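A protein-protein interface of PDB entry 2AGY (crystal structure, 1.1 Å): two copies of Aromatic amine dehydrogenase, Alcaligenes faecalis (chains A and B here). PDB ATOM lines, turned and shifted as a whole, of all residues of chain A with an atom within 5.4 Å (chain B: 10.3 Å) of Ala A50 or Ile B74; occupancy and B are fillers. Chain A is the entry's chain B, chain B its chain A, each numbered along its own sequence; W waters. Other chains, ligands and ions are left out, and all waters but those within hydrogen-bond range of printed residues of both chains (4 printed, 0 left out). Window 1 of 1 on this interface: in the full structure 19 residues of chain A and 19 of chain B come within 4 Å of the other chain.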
ATOM      1  N   LEU A  28     -18.444 -20.025 -26.415  1.00  0.00           N
ATOM      2  CA  LEU A  28     -19.145 -20.772 -25.405  1.00  0.00           C
ATOM      3  C   LEU A  28     -20.569 -20.269 -25.165  1.00  0.00           C
ATOM      4  O   LEU A  28     -21.362 -20.968 -24.567  1.00  0.00           O
ATOM      5  CB  LEU A  28     -18.324 -20.740 -24.113  1.00  0.00           C
ATOM      6  CG  LEU A  28     -18.791 -21.553 -22.916  1.00  0.00           C
ATOM      7  CD1 LEU A  28     -18.979 -23.029 -23.249  1.00  0.00           C
ATOM      8  CD2 LEU A  28     -17.790 -21.401 -21.805  1.00  0.00           C
ATOM      9  N   THR A  29     -20.884 -19.057 -25.615  1.00  0.00           N
ATOM     10  CA  THR A  29     -22.261 -18.586 -25.530  1.00  0.00           C
ATOM     11  C   THR A  29     -23.184 -19.238 -26.562  1.00  0.00           C
ATOM     12  O   THR A  29     -24.369 -18.987 -26.535  1.00  0.00           O
ATOM     13  CB  THR A  29     -22.391 -17.059 -25.680  1.00  0.00           C
ATOM     14  OG1 THR A  29     -21.962 -16.660 -27.002  1.00  0.00           O
ATOM     15  CG2 THR A  29     -21.596 -16.285 -24.640  1.00  0.00           C
ATOM     16  N   GLU A  30     -22.640 -20.060 -27.461  1.00  0.00           N
ATOM     17  CA  GLU A  30     -23.451 -20.750 -28.466  1.00  0.00           C
ATOM     18  C   GLU A  30     -23.248 -22.272 -28.410  1.00  0.00           C
ATOM     19  O   GLU A  30     -23.199 -22.961 -29.421  1.00  0.00           O
ATOM     20  CB  GLU A  30     -23.222 -20.203 -29.875  1.00  0.00           C
ATOM     21  CG  GLU A  30     -24.455 -20.415 -30.770  1.00  0.00           C
ATOM     22  CD  GLU A  30     -24.183 -20.124 -32.213  1.00  0.00           C
ATOM     23  OE1 GLU A  30     -24.348 -18.968 -32.642  1.00  0.00           O
ATOM     24  OE2 GLU A  30     -23.816 -21.064 -32.953  1.00  0.00           O
ATOM     25  N   SER A  31     -23.118 -22.770 -27.195  1.00  0.00           N
ATOM     26  CA  SER A  31     -23.111 -24.192 -26.979  1.00  0.00           C
ATOM     27  C   SER A  31     -24.426 -24.798 -27.465  1.00  0.00           C
ATOM     28  O   SER A  31     -25.434 -24.118 -27.583  1.00  0.00           O
ATOM     29  CB  SER A  31     -22.884 -24.521 -25.492  1.00  0.00           C
ATOM     30  OG  SER A  31     -24.013 -24.196 -24.678  1.00  0.00           O
ATOM     31  N   PRO A  48     -30.244 -25.681 -29.079  1.00  0.00           N
ATOM     32  CA  PRO A  48     -29.363 -24.606 -28.656  1.00  0.00           C
ATOM     33  C   PRO A  48     -29.368 -24.480 -27.149  1.00  0.00           C
ATOM     34  O   PRO A  48     -30.424 -24.594 -26.517  1.00  0.00           O
ATOM     35  CB  PRO A  48     -29.993 -23.384 -29.291  1.00  0.00           C
ATOM     36  CG  PRO A  48     -31.419 -23.698 -29.364  1.00  0.00           C
ATOM     37  CD  PRO A  48     -31.470 -25.165 -29.706  1.00  0.00           C
ATOM     38  N   THR A  49     -28.201 -24.249 -26.566  1.00  0.00           N
ATOM     39  CA  THR A  49     -28.088 -24.189 -25.103  1.00  0.00           C
ATOM     40  C   THR A  49     -27.259 -23.015 -24.587  1.00  0.00           C
ATOM     41  O   THR A  49     -26.708 -23.089 -23.499  1.00  0.00           O
ATOM     42  CB  THR A  49     -27.551 -25.514 -24.496  1.00  0.00           C
ATOM     43  OG1 THR A  49     -26.266 -25.856 -25.044  1.00  0.00           O
ATOM     44  CG2 THR A  49     -28.438 -26.677 -24.821  1.00  0.00           C
ATOM     45  N   ALA A  50     -27.185 -21.939 -25.360  1.00  0.00           N
ATOM     46  CA  ALA A  50     -26.651 -20.683 -24.863  1.00  0.00           C
ATOM     47  C   ALA A  50     -25.285 -20.871 -24.186  1.00  0.00           C
ATOM     48  O   ALA A  50     -24.419 -21.554 -24.732  1.00  0.00           O
ATOM     49  CB  ALA A  50     -27.675 -20.012 -23.957  1.00  0.00           C
ATOM     50  N   PHE A  51     -25.061 -20.251 -23.035  1.00  0.00           N
ATOM     51  CA  PHE A  51     -23.735 -20.269 -22.449  1.00  0.00           C
ATOM     52  C   PHE A  51     -23.510 -21.530 -21.659  1.00  0.00           C
ATOM     53  O   PHE A  51     -24.186 -21.760 -20.653  1.00  0.00           O
ATOM     54  CB  PHE A  51     -23.529 -19.059 -21.542  1.00  0.00           C
ATOM     55  CG  PHE A  51     -22.181 -19.016 -20.890  1.00  0.00           C
ATOM     56  CD1 PHE A  51     -21.076 -18.634 -21.599  1.00  0.00           C
ATOM     57  CD2 PHE A  51     -22.023 -19.333 -19.565  1.00  0.00           C
ATOM     58  CE1 PHE A  51     -19.833 -18.586 -20.998  1.00  0.00           C
ATOM     59  CE2 PHE A  51     -20.782 -19.289 -18.974  1.00  0.00           C
ATOM     60  CZ  PHE A  51     -19.701 -18.912 -19.689  1.00  0.00           C
ATOM     61  N   ASN A  52     -22.544 -22.329 -22.083  1.00  0.00           N
ATOM     62  CA  ASN A  52     -22.117 -23.507 -21.323  1.00  0.00           C
ATOM     63  C   ASN A  52     -23.288 -24.381 -20.910  1.00  0.00           C
ATOM     64  O   ASN A  52     -23.498 -24.646 -19.748  1.00  0.00           O
ATOM     65  CB  ASN A  52     -21.310 -23.083 -20.103  1.00  0.00           C
ATOM     66  CG  ASN A  52     -20.834 -24.260 -19.277  1.00  0.00           C
ATOM     67  OD1 ASN A  52     -20.352 -25.300 -19.820  1.00  0.00           O
ATOM     68  ND2 ASN A  52     -20.937 -24.130 -17.997  1.00  0.00           N
ATOM     69  N   GLY A  53     -24.048 -24.843 -21.881  1.00  0.00           N
ATOM     70  CA  GLY A  53     -25.166 -25.705 -21.589  1.00  0.00           C
ATOM     71  C   GLY A  53     -24.744 -27.038 -21.033  1.00  0.00           C
ATOM     72  O   GLY A  53     -23.668 -27.530 -21.327  1.00  0.00           O
ATOM     73  N   THR A  68     -28.815 -23.961 -18.535  1.00  0.00           N
ATOM     74  CA  THR A  68     -28.003 -22.937 -19.123  1.00  0.00           C
ATOM     75  C   THR A  68     -28.134 -21.617 -18.376  1.00  0.00           C
ATOM     76  O   THR A  68     -28.866 -21.517 -17.403  1.00  0.00           O
ATOM     77  CB  THR A  68     -28.299 -22.815 -20.621  1.00  0.00           C
ATOM     78  OG1 THR A  68     -27.319 -21.953 -21.204  1.00  0.00           O
ATOM     79  CG2 THR A  68     -29.668 -22.234 -20.919  1.00  0.00           C
ATOM     80  N   THR A  69     -27.364 -20.629 -18.837  1.00  0.00           N
ATOM     81  CA  THR A  69     -27.374 -19.274 -18.324  1.00  0.00           C
ATOM     82  C   THR A  69     -27.598 -18.317 -19.459  1.00  0.00           C
ATOM     83  O   THR A  69     -26.927 -18.399 -20.495  1.00  0.00           O
ATOM     84  CB  THR A  69     -26.021 -18.953 -17.670  1.00  0.00           C
ATOM     85  OG1 THR A  69     -25.843 -19.766 -16.506  1.00  0.00           O
ATOM     86  CG2 THR A  69     -25.933 -17.480 -17.232  1.00  0.00           C
ATOM     87  N   TYR A  70     -28.525 -17.397 -19.239  1.00  0.00           N
ATOM     88  CA  TYR A  70     -28.753 -16.271 -20.104  1.00  0.00           C
ATOM     89  C   TYR A  70     -28.437 -14.987 -19.349  1.00  0.00           C
ATOM     90  O   TYR A  70     -28.486 -14.942 -18.105  1.00  0.00           O
ATOM     91  CB  TYR A  70     -30.203 -16.192 -20.506  1.00  0.00           C
ATOM     92  CG  TYR A  70     -30.721 -17.369 -21.291  1.00  0.00           C
ATOM     93  CD1 TYR A  70     -31.369 -18.419 -20.661  1.00  0.00           C
ATOM     94  CD2 TYR A  70     -30.569 -17.427 -22.647  1.00  0.00           C
ATOM     95  CE1 TYR A  70     -31.860 -19.498 -21.381  1.00  0.00           C
ATOM     96  CE2 TYR A  70     -31.060 -18.503 -23.380  1.00  0.00           C
ATOM     97  CZ  TYR A  70     -31.697 -19.530 -22.744  1.00  0.00           C
ATOM     98  OH  TYR A  70     -32.188 -20.596 -23.497  1.00  0.00           O
ATOM     99  N   ILE A  74     -26.434 -10.640 -22.823  1.00  0.00           N
ATOM    100  CA  ILE A  74     -25.387 -11.667 -22.970  1.00  0.00           C
ATOM    101  C   ILE A  74     -24.195 -11.420 -22.072  1.00  0.00           C
ATOM    102  O   ILE A  74     -23.953 -12.183 -21.140  1.00  0.00           O
ATOM    103  CB  ILE A  74     -24.939 -11.859 -24.424  1.00  0.00           C
ATOM    104  CG1 ILE A  74     -26.136 -12.087 -25.347  1.00  0.00           C
ATOM    105  CG2 ILE A  74     -23.958 -13.043 -24.510  1.00  0.00           C
ATOM    106  CD1 ILE A  74     -25.796 -12.047 -26.773  1.00  0.00           C
ATOM    107  N   HIS B  27     -20.936 -19.571 -35.706  1.00  0.00           N
ATOM    108  CA  HIS B  27     -21.589 -19.318 -34.427  1.00  0.00           C
ATOM    109  C   HIS B  27     -21.986 -17.849 -34.354  1.00  0.00           C
ATOM    110  O   HIS B  27     -21.501 -17.096 -33.534  1.00  0.00           O
ATOM    111  CB  HIS B  27     -20.669 -19.727 -33.258  1.00  0.00           C
ATOM    112  CG  HIS B  27     -20.339 -21.154 -33.314  1.00  0.00           C
ATOM    113  ND1 HIS B  27     -21.288 -22.124 -33.077  1.00  0.00           N
ATOM    114  CD2 HIS B  27     -19.211 -21.797 -33.660  1.00  0.00           C
ATOM    115  CE1 HIS B  27     -20.741 -23.312 -33.254  1.00  0.00           C
ATOM    116  NE2 HIS B  27     -19.481 -23.143 -33.613  1.00  0.00           N
ATOM    117  N   LEU B  28     -22.908 -17.477 -35.247  1.00  0.00           N
ATOM    118  CA  LEU B  28     -23.163 -16.093 -35.593  1.00  0.00           C
ATOM    119  C   LEU B  28     -23.771 -15.302 -34.446  1.00  0.00           C
ATOM    120  O   LEU B  28     -23.768 -14.076 -34.485  1.00  0.00           O
ATOM    121  CB  LEU B  28     -24.091 -16.057 -36.803  1.00  0.00           C
ATOM    122  CG  LEU B  28     -24.424 -14.726 -37.446  1.00  0.00           C
ATOM    123  CD1 LEU B  28     -23.216 -13.932 -37.866  1.00  0.00           C
ATOM    124  CD2 LEU B  28     -25.293 -14.994 -38.674  1.00  0.00           C
ATOM    125  N   THR B  29     -24.292 -15.985 -33.416  1.00  0.00           N
ATOM    126  CA  THR B  29     -24.718 -15.263 -32.207  1.00  0.00           C
ATOM    127  C   THR B  29     -23.576 -14.752 -31.355  1.00  0.00           C
ATOM    128  O   THR B  29     -23.829 -14.060 -30.382  1.00  0.00           O
ATOM    129  CB  THR B  29     -25.650 -16.089 -31.313  1.00  0.00           C
ATOM    130  OG1 THR B  29     -24.966 -17.234 -30.794  1.00  0.00           O
ATOM    131  CG2 THR B  29     -26.901 -16.564 -32.057  1.00  0.00           C
ATOM    132  N   GLU B  30     -22.329 -15.095 -31.702  1.00  0.00           N
ATOM    133  CA  GLU B  30     -21.163 -14.633 -30.959  1.00  0.00           C
ATOM    134  C   GLU B  30     -20.178 -13.902 -31.845  1.00  0.00           C
ATOM    135  O   GLU B  30     -18.945 -14.010 -31.666  1.00  0.00           O
ATOM    136  CB  GLU B  30     -20.479 -15.751 -30.162  1.00  0.00           C
ATOM    137  CG  GLU B  30     -19.770 -15.220 -28.926  1.00  0.00           C
ATOM    138  CD  GLU B  30     -18.913 -16.252 -28.246  1.00  0.00           C
ATOM    139  OE1 GLU B  30     -19.412 -16.984 -27.366  1.00  0.00           O
ATOM    140  OE2 GLU B  30     -17.713 -16.327 -28.584  1.00  0.00           O
ATOM    141  N   SER B  31     -20.716 -13.129 -32.780  1.00  0.00           N
ATOM    142  CA  SER B  31     -19.900 -12.236 -33.576  1.00  0.00           C
ATOM    143  C   SER B  31     -19.189 -11.232 -32.652  1.00  0.00           C
ATOM    144  O   SER B  31     -19.624 -10.980 -31.531  1.00  0.00           O
ATOM    145  CB  SER B  31     -20.744 -11.481 -34.603  1.00  0.00           C
ATOM    146  OG  SER B  31     -21.603 -10.527 -33.994  1.00  0.00           O
ATOM    147  N   ALA B  50     -22.824  -9.928 -30.326  1.00  0.00           N
ATOM    148  CA  ALA B  50     -24.013 -10.752 -30.346  1.00  0.00           C
ATOM    149  C   ALA B  50     -24.293 -11.283 -31.748  1.00  0.00           C
ATOM    150  O   ALA B  50     -23.385 -11.759 -32.418  1.00  0.00           O
ATOM    151  CB  ALA B  50     -25.177  -9.991 -29.731  1.00  0.00           C
ATOM    152  N   PHE B  51     -25.541 -11.239 -32.200  1.00  0.00           N
ATOM    153  CA  PHE B  51     -25.898 -11.837 -33.467  1.00  0.00           C
ATOM    154  C   PHE B  51     -25.607 -10.919 -34.628  1.00  0.00           C
ATOM    155  O   PHE B  51     -26.201  -9.870 -34.760  1.00  0.00           O
ATOM    156  CB  PHE B  51     -27.386 -12.237 -33.483  1.00  0.00           C
ATOM    157  CG  PHE B  51     -27.818 -12.870 -34.780  1.00  0.00           C
ATOM    158  CD1 PHE B  51     -27.487 -14.189 -35.070  1.00  0.00           C
ATOM    159  CD2 PHE B  51     -28.547 -12.159 -35.712  1.00  0.00           C
ATOM    160  CE1 PHE B  51     -27.879 -14.770 -36.262  1.00  0.00           C
ATOM    161  CE2 PHE B  51     -28.939 -12.761 -36.911  1.00  0.00           C
ATOM    162  CZ  PHE B  51     -28.601 -14.061 -37.163  1.00  0.00           C
ATOM    163  N   ASN B  52     -24.693 -11.336 -35.490  1.00  0.00           N
ATOM    164  CA  ASN B  52     -24.416 -10.609 -36.728  1.00  0.00           C
ATOM    165  C   ASN B  52     -24.188  -9.115 -36.476  1.00  0.00           C
ATOM    166  O   ASN B  52     -24.887  -8.264 -37.030  1.00  0.00           O
ATOM    167  CB  ASN B  52     -25.566 -10.822 -37.750  1.00  0.00           C
ATOM    168  CG  ASN B  52     -25.331 -10.099 -39.047  1.00  0.00           C
ATOM    169  OD1 ASN B  52     -24.194 -10.089 -39.617  1.00  0.00           O
ATOM    170  ND2 ASN B  52     -26.365  -9.511 -39.553  1.00  0.00           N
ATOM    171  N   THR B  68     -26.516  -4.455 -33.469  1.00  0.00           N
ATOM    172  CA  THR B  68     -26.754  -5.875 -33.300  1.00  0.00           C
ATOM    173  C   THR B  68     -28.188  -6.157 -32.928  1.00  0.00           C
ATOM    174  O   THR B  68     -28.999  -5.243 -32.817  1.00  0.00           O
ATOM    175  CB  THR B  68     -25.755  -6.454 -32.279  1.00  0.00           C
ATOM    176  OG1 THR B  68     -25.856  -7.888 -32.295  1.00  0.00           O
ATOM    177  CG2 THR B  68     -26.023  -5.983 -30.845  1.00  0.00           C
ATOM    178  N   THR B  69     -28.484  -7.446 -32.778  1.00  0.00           N
ATOM    179  CA  THR B  69     -29.797  -7.931 -32.388  1.00  0.00           C
ATOM    180  C   THR B  69     -29.640  -8.854 -31.218  1.00  0.00           C
ATOM    181  O   THR B  69     -28.810  -9.754 -31.242  1.00  0.00           O
ATOM    182  CB  THR B  69     -30.424  -8.716 -33.559  1.00  0.00           C
ATOM    183  OG1 THR B  69     -30.703  -7.829 -34.644  1.00  0.00           O
ATOM    184  CG2 THR B  69     -31.770  -9.404 -33.158  1.00  0.00           C
ATOM    185  N   TYR B  70     -30.476  -8.630 -30.212  1.00  0.00           N
ATOM    186  CA  TYR B  70     -30.631  -9.516 -29.079  1.00  0.00           C
ATOM    187  C   TYR B  70     -32.044 -10.087 -29.084  1.00  0.00           C
ATOM    188  O   TYR B  70     -32.952  -9.490 -29.635  1.00  0.00           O
ATOM    189  CB  TYR B  70     -30.466  -8.740 -27.785  1.00  0.00           C
ATOM    190  CG  TYR B  70     -29.129  -8.120 -27.574  1.00  0.00           C
ATOM    191  CD1 TYR B  70     -28.906  -6.796 -27.891  1.00  0.00           C
ATOM    192  CD2 TYR B  70     -28.080  -8.853 -27.040  1.00  0.00           C
ATOM    193  CE1 TYR B  70     -27.663  -6.209 -27.695  1.00  0.00           C
ATOM    194  CE2 TYR B  70     -26.826  -8.270 -26.838  1.00  0.00           C
ATOM    195  CZ  TYR B  70     -26.639  -6.950 -27.168  1.00  0.00           C
ATOM    196  OH  TYR B  70     -25.418  -6.339 -26.963  1.00  0.00           O
ATOM    197  N   HIS B  71     -32.208 -11.241 -28.454  1.00  0.00           N
ATOM    198  CA  HIS B  71     -33.518 -11.725 -28.030  1.00  0.00           C
ATOM    199  C   HIS B  71     -33.431 -12.156 -26.574  1.00  0.00           C
ATOM    200  O   HIS B  71     -32.390 -12.570 -26.104  1.00  0.00           O
ATOM    201  CB  HIS B  71     -33.980 -12.926 -28.866  1.00  0.00           C
ATOM    202  CG  HIS B  71     -34.287 -12.614 -30.294  1.00  0.00           C
ATOM    203  ND1 HIS B  71     -33.322 -12.564 -31.270  1.00  0.00           N
ATOM    204  CD2 HIS B  71     -35.463 -12.348 -30.910  1.00  0.00           C
ATOM    205  CE1 HIS B  71     -33.895 -12.281 -32.430  1.00  0.00           C
ATOM    206  NE2 HIS B  71     -35.193 -12.142 -32.235  1.00  0.00           N
ATOM    207  N   GLU B  72     -34.546 -12.079 -25.868  1.00  0.00           N
ATOM    208  CA  GLU B  72     -34.533 -12.365 -24.430  1.00  0.00           C
ATOM    209  C   GLU B  72     -33.923 -13.724 -24.109  1.00  0.00           C
ATOM    210  O   GLU B  72     -33.270 -13.896 -23.079  1.00  0.00           O
ATOM    211  CB  GLU B  72     -35.929 -12.338 -23.874  1.00  0.00           C
ATOM    212  CG  GLU B  72     -36.627 -11.006 -23.882  1.00  0.00           C
ATOM    213  CD  GLU B  72     -38.059 -11.139 -23.408  1.00  0.00           C
ATOM    214  OE1 GLU B  72     -38.879 -11.852 -24.083  1.00  0.00           O
ATOM    215  OE2 GLU B  72     -38.383 -10.539 -22.364  1.00  0.00           O
ATOM    216  N   ARG B  73     -34.151 -14.697 -24.991  1.00  0.00           N
ATOM    217  CA  ARG B  73     -33.590 -16.027 -24.807  1.00  0.00           C
ATOM    218  C   ARG B  73     -32.892 -16.503 -26.071  1.00  0.00           C
ATOM    219  O   ARG B  73     -32.850 -17.684 -26.341  1.00  0.00           O
ATOM    220  CB  ARG B  73     -34.684 -16.988 -24.361  1.00  0.00           C
ATOM    221  CG  ARG B  73     -35.224 -16.679 -22.986  1.00  0.00           C
ATOM    222  CD  ARG B  73     -34.320 -17.143 -21.905  1.00  0.00           C
ATOM    223  NE  ARG B  73     -34.925 -17.010 -20.605  1.00  0.00           N
ATOM    224  CZ  ARG B  73     -34.908 -15.921 -19.883  1.00  0.00           C
ATOM    225  NH1 ARG B  73     -34.297 -14.831 -20.308  1.00  0.00           N
ATOM    226  NH2 ARG B  73     -35.510 -15.921 -18.704  1.00  0.00           N
ATOM    227  N   ILE B  74     -32.325 -15.539 -26.808  1.00  0.00           N
ATOM    228  CA  ILE B  74     -31.467 -15.752 -27.988  1.00  0.00           C
ATOM    229  C   ILE B  74     -32.242 -16.271 -29.176  1.00  0.00           C
ATOM    230  O   ILE B  74     -32.389 -15.573 -30.157  1.00  0.00           O
ATOM    231  CB  ILE B  74     -30.242 -16.626 -27.682  1.00  0.00           C
ATOM    232  CG1 ILE B  74     -29.499 -16.118 -26.453  1.00  0.00           C
ATOM    233  CG2 ILE B  74     -29.321 -16.629 -28.881  1.00  0.00           C
ATOM    234  CD1 ILE B  74     -28.501 -17.055 -25.911  1.00  0.00           C
ATOM    235  N   THR B  75     -32.738 -17.503 -29.061  1.00  0.00           N
ATOM    236  CA  THR B  75     -33.487 -18.164 -30.128  1.00  0.00           C
ATOM    237  C   THR B  75     -35.014 -18.102 -29.920  1.00  0.00           C
ATOM    238  O   THR B  75     -35.776 -18.623 -30.723  1.00  0.00           O
ATOM    239  CB  THR B  75     -33.041 -19.621 -30.248  1.00  0.00           C
ATOM    240  OG1 THR B  75     -32.915 -20.206 -28.946  1.00  0.00           O
ATOM    241  CG2 THR B  75     -31.661 -19.714 -30.852  1.00  0.00           C
ATOM    242  N   ARG B  76     -35.425 -17.454 -28.826  1.00  0.00           N
ATOM    243  CA  ARG B  76     -36.823 -17.170 -28.580  1.00  0.00           C
ATOM    244  C   ARG B  76     -36.888 -15.907 -27.722  1.00  0.00           C
ATOM    245  O   ARG B  76     -35.866 -15.442 -27.193  1.00  0.00           O
ATOM    246  CB  ARG B  76     -37.523 -18.351 -27.887  1.00  0.00           C
ATOM    247  CG  ARG B  76     -36.955 -18.719 -26.562  1.00  0.00           C
ATOM    248  CD  ARG B  76     -37.564 -19.990 -25.948  1.00  0.00           C
ATOM    249  NE  ARG B  76     -36.826 -20.329 -24.753  1.00  0.00           N
ATOM    250  CZ  ARG B  76     -37.099 -19.862 -23.559  1.00  0.00           C
ATOM    251  NH1 ARG B  76     -38.122 -19.054 -23.380  1.00  0.00           N
ATOM    252  NH2 ARG B  76     -36.338 -20.212 -22.528  1.00  0.00           N
ATOM    253  N   GLY B  77     -38.082 -15.372 -27.599  1.00  0.00           N
ATOM    254  CA  GLY B  77     -38.329 -14.200 -26.804  1.00  0.00           C
ATOM    255  C   GLY B  77     -38.218 -12.925 -27.609  1.00  0.00           C
ATOM    256  O   GLY B  77     -37.935 -12.943 -28.793  1.00  0.00           O
ATOM    257  N   LYS B  78     -38.441 -11.810 -26.941  1.00  0.00           N
ATOM    258  CA  LYS B  78     -38.580 -10.543 -27.611  1.00  0.00           C
ATOM    259  C   LYS B  78     -37.257 -10.087 -28.228  1.00  0.00           C
ATOM    260  O   LYS B  78     -36.195 -10.204 -27.614  1.00  0.00           O
ATOM    261  CB  LYS B  78     -39.089  -9.480 -26.641  1.00  0.00           C
ATOM    262  CG  LYS B  78     -39.278  -8.110 -27.282  1.00  0.00           C
ATOM    263  CD  LYS B  78     -39.929  -7.129 -26.340  1.00  0.00           C
ATOM    264  CE  LYS B  78     -40.331  -5.855 -27.064  1.00  0.00           C
ATOM    265  NZ  LYS B  78     -40.085  -4.652 -26.217  1.00  0.00           N
ATOM    266  N   ARG B  79     -37.370  -9.571 -29.449  1.00  0.00           N
ATOM    267  CA  ARG B  79     -36.255  -9.001 -30.184  1.00  0.00           C
ATOM    268  C   ARG B  79     -35.961  -7.568 -29.758  1.00  0.00           C
ATOM    269  O   ARG B  79     -36.867  -6.760 -29.582  1.00  0.00           O
ATOM    270  CB  ARG B  79     -36.601  -9.010 -31.656  1.00  0.00           C
ATOM    271  CG  ARG B  79     -35.532  -8.441 -32.590  1.00  0.00           C
ATOM    272  CD  ARG B  79     -35.788  -8.828 -34.027  1.00  0.00           C
ATOM    273  NE  ARG B  79     -34.966  -8.068 -34.952  1.00  0.00           N
ATOM    274  CZ  ARG B  79     -34.965  -8.263 -36.264  1.00  0.00           C
ATOM    275  NH1 ARG B  79     -35.736  -9.191 -36.808  1.00  0.00           N
ATOM    276  NH2 ARG B  79     -34.206  -7.524 -37.035  1.00  0.00           N
ATOM    277  N   SER B  80     -34.677  -7.267 -29.614  1.00  0.00           N
ATOM    278  CA  SER B  80     -34.197  -5.906 -29.461  1.00  0.00           C
ATOM    279  C   SER B  80     -33.064  -5.651 -30.442  1.00  0.00           C
ATOM    280  O   SER B  80     -31.962  -6.197 -30.276  1.00  0.00           O
ATOM    281  CB  SER B  80     -33.657  -5.669 -28.048  1.00  0.00           C
ATOM    282  OG  SER B  80     -34.634  -5.903 -27.052  1.00  0.00           O
ATOM    283  N   ASP B  81     -33.318  -4.815 -31.438  1.00  0.00           N
ATOM    284  CA  ASP B  81     -32.284  -4.311 -32.312  1.00  0.00           C
ATOM    285  C   ASP B  81     -31.757  -3.020 -31.688  1.00  0.00           C
ATOM    286  O   ASP B  81     -32.521  -2.183 -31.219  1.00  0.00           O
ATOM    287  CB  ASP B  81     -32.834  -4.004 -33.702  1.00  0.00           C
ATOM    288  CG  ASP B  81     -33.114  -5.224 -34.520  1.00  0.00           C
ATOM    289  OD1 ASP B  81     -32.870  -6.369 -34.033  1.00  0.00           O
ATOM    290  OD2 ASP B  81     -33.586  -5.093 -35.664  1.00  0.00           O
ATOM    291  N   GLN B 105     -29.868  -7.497 -41.197  1.00  0.00           N
ATOM    292  CA  GLN B 105     -29.097  -8.656 -40.833  1.00  0.00           C
ATOM    293  C   GLN B 105     -28.516  -9.186 -42.115  1.00  0.00           C
ATOM    294  O   GLN B 105     -29.212  -9.602 -43.001  1.00  0.00           O
ATOM    295  CB  GLN B 105     -29.965  -9.680 -40.111  1.00  0.00           C
ATOM    296  CG  GLN B 105     -30.511  -9.132 -38.809  1.00  0.00           C
ATOM    297  CD  GLN B 105     -31.437 -10.079 -38.076  1.00  0.00           C
ATOM    298  OE1 GLN B 105     -31.704  -9.893 -36.872  1.00  0.00           O
ATOM    299  NE2 GLN B 105     -31.912 -11.059 -38.743  1.00  0.00           N
HETATM  300  O   HOH W   1     -32.478 -20.300 -25.930  1.00  0.00           O
HETATM  301  O   HOH W   2     -23.132 -14.298 -27.718  1.00  0.00           O
HETATM  302  O   HOH W   3     -34.429 -21.889 -25.476  1.00  0.00           O
HETATM  303  O   HOH W   4     -26.112 -18.079 -28.454  1.00  0.00           O
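A ring nitrogen (ND1) of His B27 is in hydrogen-bond range of the side-chain carboxylate of Glu A30 (2.7 Å).
The backbone NH (N) of Leu B28 sits at hydrogen-bond distance from the side-chain carboxylate (OE1) of Glu A30 (3.3 Å).
The side-chain hydroxyl (OG1) of Thr B29 lies within hydrogen-bond range of the side-chain carboxylate (OE1) of Glu A30, at 2.6 Å.
OE1 of Glu B30 is in hydrogen-bond range of N of Leu A28 (3.3 Å).
OE1 of Glu B30 sits at hydrogen-bond distance from OG1 of Thr A29 (2.6 Å).
OG1 of Thr B75 touches CG of Pro A48, at 3.8 Å.
Ile B74 touches Ala A50 (CD1 to CB, 3.6 Å).
CE1 of Tyr A70 touches CD of Arg B73, at 3.4 Å.
Tyr A70 touches Ile B74.
Ala B50 touches Ile A74.
CD1 of Ile A74 touches CE2 of Tyr B70, at 3.9 Å.
Leu A28 touches Glu B30, and with the chains exchanged Glu A30 touches Leu B28.
Thr A29 touches Glu B30, and with the chains exchanged Glu A30 touches Thr B29.
Ala A50 touches Ile B74, and with the chains exchanged Ile A74 touches Ala B50.
Tyr A70 touches Ile B74, and with the chains exchanged Ile A74 touches Tyr B70.
Of the 11 pairs that touch across the chains among the printed residues, 8 have their exchanged pair printed and touching as well.
The backbone carbonyl oxygen (O) of Leu B28 lies within hydrogen-bond range of the backbone NH (N) of Asn B52, at 3.1 Å.
The side-chain hydroxyl (OG) of Ser B31 sits at hydrogen-bond distance from the backbone carbonyl oxygen (O) of Ala B50 (2.7 Å).
O of Tyr B70 lies within hydrogen-bond range of N of Ser B80 (2.8 Å).
The backbone carbonyl oxygen of Ile B74 lies within hydrogen-bond range of a ring nitrogen (ND1) of His B71 (3.3 Å).
O of Leu A28 is in hydrogen-bond range of N of Asn A52 (3.1 Å).
The side-chain hydroxyl (OG) of Ser A31 is in hydrogen-bond range of the backbone carbonyl oxygen (O) of Ala A50.
Water W1 lies within hydrogen-bond range of the side-chain hydroxyl of Tyr A70, the backbone carbonyl oxygen of Arg B73 and the side-chain hydroxyl of Thr B75.
Water W2 lies within hydrogen-bond range of OG1 of Thr A29 (2.7 Å) and O of Thr B29 (2.8 Å).
Water W4 bridges OG1 of Thr B29 and O of Thr A29.
Water W3 bridges the guanidinium group (NE) of Arg B76 and the side-chain hydroxyl (OH) of Tyr A70.
Printed residues of chain B within 4 Å of Leu A28: Glu B30 (3.3 Å).
Printed residues of chain B within 4 Å of Glu A30: His B27 (2.7 Å), Leu B28 (3.3 Å) and Thr B29 (2.6 Å).
No residue of chain B comes within 4 Å of Ser A31.
Ala A50 touches one residue of chain B.
Gly A53 touches none of the printed residues of chain B.
Of the printed residues of chain B, Tyr A70 touches Arg B73 (3.4 Å) and Ile B74 (3.9 Å).
Printed residues of chain A within 4 Å of Tyr B70: Ile A74 (3.9 Å).
Ile B74 touches just these residues of chain A: Ala A50 and Tyr A70.
Of the printed residues of chain A, Thr B75 touches Pro A48.
Gln B105 touches none of the printed residues of chain A.
The nearest residue of chain A that does not touch Ile B74 is Thr A29 (4.6 Å).
Of the 14 printed residues of chain A, 7 touch a printed residue of chain B.
Hydrophobic or aromatic side chains of chain A that line the printed part of chain B: Pro A48, Ala A50, Tyr A70 and Ile A74.
Along chain B the printed residues that touch a printed residue of chain A span positions 27 to 75.
Among the printed residues, no Asp or Glu carboxylate lies within 4 Å of a Lys or Arg side-chain nitrogen of the other chain.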
